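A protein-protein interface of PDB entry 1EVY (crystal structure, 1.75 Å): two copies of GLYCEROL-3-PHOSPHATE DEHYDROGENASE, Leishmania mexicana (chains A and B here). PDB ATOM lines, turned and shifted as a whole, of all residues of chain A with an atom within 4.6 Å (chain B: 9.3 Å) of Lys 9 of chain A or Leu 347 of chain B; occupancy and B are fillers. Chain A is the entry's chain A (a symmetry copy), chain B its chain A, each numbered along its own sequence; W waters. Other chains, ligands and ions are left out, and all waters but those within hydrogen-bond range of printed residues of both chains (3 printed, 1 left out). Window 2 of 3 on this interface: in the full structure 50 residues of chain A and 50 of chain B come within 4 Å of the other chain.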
ATOM      1  N   LYS A   9     -17.582 -23.834   2.746  1.00  0.00           N
ATOM      2  CA  LYS A   9     -17.504 -23.357   4.130  1.00  0.00           C
ATOM      3  C   LYS A   9     -18.854 -23.405   4.870  1.00  0.00           C
ATOM      4  O   LYS A   9     -19.748 -22.569   4.636  1.00  0.00           O
ATOM      5  CB  LYS A   9     -16.822 -21.957   4.223  1.00  0.00           C
ATOM      6  CG  LYS A   9     -15.948 -21.746   5.496  1.00  0.00           C
ATOM      7  N   ASP A  10     -18.988 -24.390   5.775  1.00  0.00           N
ATOM      8  CA  ASP A  10     -20.217 -24.546   6.548  1.00  0.00           C
ATOM      9  C   ASP A  10     -20.236 -23.663   7.783  1.00  0.00           C
ATOM     10  O   ASP A  10     -21.163 -23.745   8.612  1.00  0.00           O
ATOM     11  CB  ASP A  10     -20.589 -25.997   6.901  1.00  0.00           C
ATOM     12  CG  ASP A  10     -20.147 -26.968   5.846  1.00  0.00           C
ATOM     13  OD1 ASP A  10     -19.045 -26.908   5.342  1.00  0.00           O
ATOM     14  OD2 ASP A  10     -21.084 -27.794   5.428  1.00  0.00           O
ATOM     15  N   GLU A  11     -19.203 -22.822   7.851  1.00  0.00           N
ATOM     16  CA  GLU A  11     -19.001 -21.890   8.930  1.00  0.00           C
ATOM     17  C   GLU A  11     -19.939 -20.695   8.828  1.00  0.00           C
ATOM     18  O   GLU A  11     -19.986 -19.953   7.839  1.00  0.00           O
ATOM     19  CB  GLU A  11     -17.537 -21.473   8.827  1.00  0.00           C
ATOM     20  CG  GLU A  11     -16.769 -21.258  10.147  1.00  0.00           C
ATOM     21  CD  GLU A  11     -15.420 -20.613   9.844  1.00  0.00           C
ATOM     22  OE1 GLU A  11     -15.229 -19.386   9.885  1.00  0.00           O
ATOM     23  OE2 GLU A  11     -14.493 -21.488   9.466  1.00  0.00           O
ATOM     24  N   LEU A  12     -20.713 -20.459   9.878  1.00  0.00           N
ATOM     25  CA  LEU A  12     -21.656 -19.350   9.823  1.00  0.00           C
ATOM     26  C   LEU A  12     -20.957 -18.007   9.724  1.00  0.00           C
ATOM     27  O   LEU A  12     -19.775 -17.926   9.981  1.00  0.00           O
ATOM     28  CB  LEU A  12     -22.633 -19.336  11.034  1.00  0.00           C
ATOM     29  CG  LEU A  12     -23.363 -20.668  11.248  1.00  0.00           C
ATOM     30  CD1 LEU A  12     -24.493 -20.545  12.288  1.00  0.00           C
ATOM     31  CD2 LEU A  12     -23.952 -21.014   9.903  1.00  0.00           C
ATOM     32  N   GLN A 182     -26.509 -17.889   2.699  1.00  0.00           N
ATOM     33  CA  GLN A 182     -26.783 -19.083   3.431  1.00  0.00           C
ATOM     34  C   GLN A 182     -26.087 -19.042   4.790  1.00  0.00           C
ATOM     35  O   GLN A 182     -26.646 -19.413   5.811  1.00  0.00           O
ATOM     36  CB  GLN A 182     -26.161 -20.247   2.653  1.00  0.00           C
ATOM     37  CG  GLN A 182     -27.060 -21.465   2.517  1.00  0.00           C
ATOM     38  CD  GLN A 182     -26.390 -22.678   1.928  1.00  0.00           C
ATOM     39  OE1 GLN A 182     -25.501 -22.614   1.094  1.00  0.00           O
ATOM     40  NE2 GLN A 182     -26.892 -23.834   2.294  1.00  0.00           N
ATOM     41  N   ARG A 183     -24.823 -18.648   4.786  1.00  0.00           N
ATOM     42  CA  ARG A 183     -23.988 -18.549   5.967  1.00  0.00           C
ATOM     43  C   ARG A 183     -24.442 -17.440   6.890  1.00  0.00           C
ATOM     44  O   ARG A 183     -24.144 -17.468   8.065  1.00  0.00           O
ATOM     45  CB  ARG A 183     -22.560 -18.362   5.492  1.00  0.00           C
ATOM     46  CG  ARG A 183     -22.036 -19.660   4.867  1.00  0.00           C
ATOM     47  CD  ARG A 183     -20.740 -19.480   4.117  1.00  0.00           C
ATOM     48  NE  ARG A 183     -20.016 -18.399   4.709  1.00  0.00           N
ATOM     49  CZ  ARG A 183     -18.835 -18.515   5.243  1.00  0.00           C
ATOM     50  NH1 ARG A 183     -18.187 -19.667   5.247  1.00  0.00           N
ATOM     51  NH2 ARG A 183     -18.279 -17.443   5.783  1.00  0.00           N
ATOM     52  N   SER A 186     -28.549 -18.715   8.197  1.00  0.00           N
ATOM     53  CA  SER A 186     -28.628 -19.945   8.985  1.00  0.00           C
ATOM     54  C   SER A 186     -28.235 -19.785  10.458  1.00  0.00           C
ATOM     55  O   SER A 186     -27.166 -19.228  10.717  1.00  0.00           O
ATOM     56  CB  SER A 186     -27.676 -20.991   8.390  1.00  0.00           C
ATOM     57  OG  SER A 186     -28.141 -21.336   7.082  1.00  0.00           O
ATOM     58  N   ARG A 190     -29.037 -24.392  14.540  1.00  0.00           N
ATOM     59  CA  ARG A 190     -29.595 -25.237  13.475  1.00  0.00           C
ATOM     60  C   ARG A 190     -31.135 -25.246  13.494  1.00  0.00           C
ATOM     61  O   ARG A 190     -31.724 -26.265  13.121  1.00  0.00           O
ATOM     62  CB  ARG A 190     -29.135 -26.681  13.548  1.00  0.00           C
ATOM     63  CG  ARG A 190     -27.621 -26.873  13.565  1.00  0.00           C
ATOM     64  CD  ARG A 190     -26.910 -26.354  12.326  1.00  0.00           C
ATOM     65  NE  ARG A 190     -26.945 -27.258  11.169  1.00  0.00           N
ATOM     66  CZ  ARG A 190     -27.124 -26.863   9.885  1.00  0.00           C
ATOM     67  NH1 ARG A 190     -27.295 -25.560   9.553  1.00  0.00           N
ATOM     68  NH2 ARG A 190     -27.161 -27.809   8.915  1.00  0.00           N
ATOM     69  N   LEU B 342     -28.450 -35.863  12.034  1.00  0.00           N
ATOM     70  CA  LEU B 342     -29.022 -35.542  10.761  1.00  0.00           C
ATOM     71  C   LEU B 342     -28.593 -34.141  10.417  1.00  0.00           C
ATOM     72  O   LEU B 342     -28.248 -33.861   9.284  1.00  0.00           O
ATOM     73  CB  LEU B 342     -30.528 -35.464  10.965  1.00  0.00           C
ATOM     74  CG  LEU B 342     -31.431 -36.174   9.970  1.00  0.00           C
ATOM     75  CD1 LEU B 342     -32.585 -35.256   9.644  1.00  0.00           C
ATOM     76  CD2 LEU B 342     -30.741 -36.598   8.678  1.00  0.00           C
ATOM     77  N   LEU B 343     -28.642 -33.231  11.398  1.00  0.00           N
ATOM     78  CA  LEU B 343     -28.273 -31.867  11.056  1.00  0.00           C
ATOM     79  C   LEU B 343     -26.806 -31.628  10.936  1.00  0.00           C
ATOM     80  O   LEU B 343     -26.401 -30.534  10.626  1.00  0.00           O
ATOM     81  CB  LEU B 343     -28.931 -30.768  11.896  1.00  0.00           C
ATOM     82  CG  LEU B 343     -30.451 -30.881  11.845  1.00  0.00           C
ATOM     83  CD1 LEU B 343     -31.076 -30.071  12.943  1.00  0.00           C
ATOM     84  CD2 LEU B 343     -30.949 -30.366  10.520  1.00  0.00           C
ATOM     85  N   SER B 344     -26.024 -32.655  11.168  1.00  0.00           N
ATOM     86  CA  SER B 344     -24.578 -32.500  11.118  1.00  0.00           C
ATOM     87  C   SER B 344     -23.965 -32.303   9.747  1.00  0.00           C
ATOM     88  O   SER B 344     -22.789 -32.016   9.621  1.00  0.00           O
ATOM     89  CB  SER B 344     -23.847 -33.614  11.878  1.00  0.00           C
ATOM     90  OG  SER B 344     -23.813 -34.827  11.119  1.00  0.00           O
ATOM     91  N   CYS B 345     -24.716 -32.458   8.700  1.00  0.00           N
ATOM     92  CA  CYS B 345     -24.143 -32.311   7.368  1.00  0.00           C
ATOM     93  C   CYS B 345     -23.533 -30.947   6.984  1.00  0.00           C
ATOM     94  O   CYS B 345     -22.827 -30.870   6.007  1.00  0.00           O
ATOM     95  CB  CYS B 345     -25.210 -32.705   6.333  1.00  0.00           C
ATOM     96  SG  CYS B 345     -26.767 -31.854   6.706  1.00  0.00           S
ATOM     97  N   GLY B 346     -23.780 -29.817   7.650  1.00  0.00           N
ATOM     98  CA  GLY B 346     -23.156 -28.629   7.096  1.00  0.00           C
ATOM     99  C   GLY B 346     -24.101 -27.880   6.178  1.00  0.00           C
ATOM    100  O   GLY B 346     -25.310 -28.108   6.169  1.00  0.00           O
ATOM    101  N   LEU B 347     -23.579 -26.933   5.436  1.00  0.00           N
ATOM    102  CA  LEU B 347     -24.456 -26.159   4.600  1.00  0.00           C
ATOM    103  C   LEU B 347     -24.486 -26.734   3.218  1.00  0.00           C
ATOM    104  O   LEU B 347     -23.469 -27.079   2.659  1.00  0.00           O
ATOM    105  CB  LEU B 347     -24.047 -24.685   4.519  1.00  0.00           C
ATOM    106  CG  LEU B 347     -24.000 -23.953   5.853  1.00  0.00           C
ATOM    107  CD1 LEU B 347     -23.349 -22.582   5.657  1.00  0.00           C
ATOM    108  CD2 LEU B 347     -25.414 -23.679   6.296  1.00  0.00           C
ATOM    109  N   GLN B 348     -25.644 -26.816   2.598  1.00  0.00           N
ATOM    110  CA  GLN B 348     -25.556 -27.374   1.263  1.00  0.00           C
ATOM    111  C   GLN B 348     -26.530 -26.812   0.287  1.00  0.00           C
ATOM    112  O   GLN B 348     -27.417 -26.028   0.588  1.00  0.00           O
ATOM    113  CB  GLN B 348     -25.790 -28.867   1.176  1.00  0.00           C
ATOM    114  CG  GLN B 348     -25.775 -29.596   2.516  1.00  0.00           C
ATOM    115  CD  GLN B 348     -25.331 -30.982   2.228  1.00  0.00           C
ATOM    116  OE1 GLN B 348     -26.088 -31.961   2.422  1.00  0.00           O
ATOM    117  NE2 GLN B 348     -24.118 -31.017   1.676  1.00  0.00           N
ATOM    118  N   ASP B 349     -26.317 -27.264  -0.926  1.00  0.00           N
ATOM    119  CA  ASP B 349     -27.167 -26.881  -2.018  1.00  0.00           C
ATOM    120  C   ASP B 349     -28.354 -27.850  -1.962  1.00  0.00           C
ATOM    121  O   ASP B 349     -28.231 -28.982  -1.497  1.00  0.00           O
ATOM    122  CB  ASP B 349     -26.387 -27.083  -3.344  1.00  0.00           C
ATOM    123  CG  ASP B 349     -25.229 -26.112  -3.568  1.00  0.00           C
ATOM    124  OD1 ASP B 349     -24.896 -25.188  -2.797  1.00  0.00           O
ATOM    125  OD2 ASP B 349     -24.656 -26.332  -4.723  1.00  0.00           O
ATOM    126  N   GLU B 350     -29.482 -27.392  -2.427  1.00  0.00           N
ATOM    127  CA  GLU B 350     -30.669 -28.206  -2.428  1.00  0.00           C
ATOM    128  C   GLU B 350     -30.556 -29.586  -3.069  1.00  0.00           C
ATOM    129  O   GLU B 350     -31.179 -30.529  -2.613  1.00  0.00           O
ATOM    130  CB  GLU B 350     -31.809 -27.412  -3.020  1.00  0.00           C
ATOM    131  CG  GLU B 350     -33.132 -27.897  -2.467  1.00  0.00           C
ATOM    132  CD  GLU B 350     -34.264 -26.918  -2.654  1.00  0.00           C
ATOM    133  OE1 GLU B 350     -34.422 -26.106  -3.586  1.00  0.00           O
ATOM    134  OE2 GLU B 350     -35.143 -27.146  -1.734  1.00  0.00           O
HETATM  135  O   HOH W   1     -24.785 -28.557  12.814  1.00  0.00           O
HETATM  136  O   HOH W   2     -20.532 -27.507   2.743  1.00  0.00           O
HETATM  137  O   HOH W   3     -28.004 -26.477   4.071  1.00  0.00           O
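Lys 9 of chain A touches just one residue of chain B: Leu 347 (3.7 Å).
Asp 10 of chain A touches just these residues of chain B: Cys 345, Gly 346 and Leu 347.
No residue of chain B comes within 4 Å of Glu 11 of chain A.
Of the printed residues of chain B, Arg 183 of chain A touches Leu 347 (3.3 Å).
Printed residues of chain A within 4 Å of Leu 343 of chain B: Arg 190 (3.3 Å).
Ser 344 of chain B touches none of the printed residues of chain A.
Printed residues of chain A within 4 Å of Gly 346 of chain B: Asp 10 (2.8 Å) and Arg 190 (3.3 Å).
Leu 347 of chain B touches five residues of chain A.
Asp 349 of chain B touches none of the printed residues of chain A.
The nearest residue of chain B that does not touch Lys 9 of chain A is Gly 346 of chain B (7.0 Å).
The nearest residue of chain A that does not touch Leu 347 of chain B is Arg 190 of chain A (4.2 Å).
O of Lys 9 of chain A touches CD1 of Leu 347 of chain B (3.7 Å).
OD2 of Asp 10 of chain A touches O of Cys 345 of chain B (3.6 Å).
CA of Gly 346 of chain B touches OD2 of Asp 10 of chain A (2.8 Å).
CB of Leu 347 of chain B touches NE2 of Gln 182 of chain A, at 3.7 Å.
CD1 of Leu 347 of chain B touches CG of Arg 183 of chain A, 3.3 Å away.
CD2 of Leu 347 of chain B touches OG of Ser 186 of chain A (3.7 Å).
Water W2 lies within hydrogen-bond range of the side-chain carboxylate (OD2) of Asp 10 of chain A (2.8 Å) and the backbone carbonyl oxygen (O) of Leu 347 of chain B (3.0 Å).
Water W3 lies within hydrogen-bond range of N of Gln 348 of chain B and NE2 of Gln 182 of chain A.
Water W1 bridges the guanidinium group (NE) of Arg 190 of chain A (3.0 Å) and the backbone carbonyl oxygen (O) of Leu 343 of chain B (3.4 Å).
The backbone NH of Leu 347 of chain B lies within hydrogen-bond range of the side-chain carboxylate of Asp 10 of chain A, at 2.6 Å.
The guanidinium group (NH2) of Arg 190 of chain A lies within hydrogen-bond range of the backbone carbonyl oxygen (O) of Gly 346 of chain B, at 3.3 Å.
NE2 of Gln 182 of chain A lies within hydrogen-bond range of O of Gln 348 of chain B (2.8 Å).
The backbone carbonyl oxygen of Leu 343 of chain B is in hydrogen-bond range of the guanidinium group of Arg 190 of chain A, 3.3 Å away.
OG of Ser 186 of chain A lies within hydrogen-bond range of O of Gln 182 of chain A.
The side-chain sulfur (SG) of Cys 345 of chain B is in hydrogen-bond range of the backbone carbonyl oxygen (O) of Leu 342 of chain B.
The backbone carbonyl oxygen (O) of Lys 9 of chain A lies close to the guanidinium group (NH1) of Arg 183 of chain A (3.4 Å).
O of Glu 11 of chain A sits at hydrogen-bond distance from NH1 of Arg 183 of chain A, at 3.2 Å.
No position is printed for both chains.
Of the 8 printed residues of chain A, 6 touch a printed residue of chain B.
Hydrophobic or aromatic side chains of chain B that line the printed part of chain A: Leu 343 and Leu 347.
Among the printed residues, 10 pairs touch across the chains.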
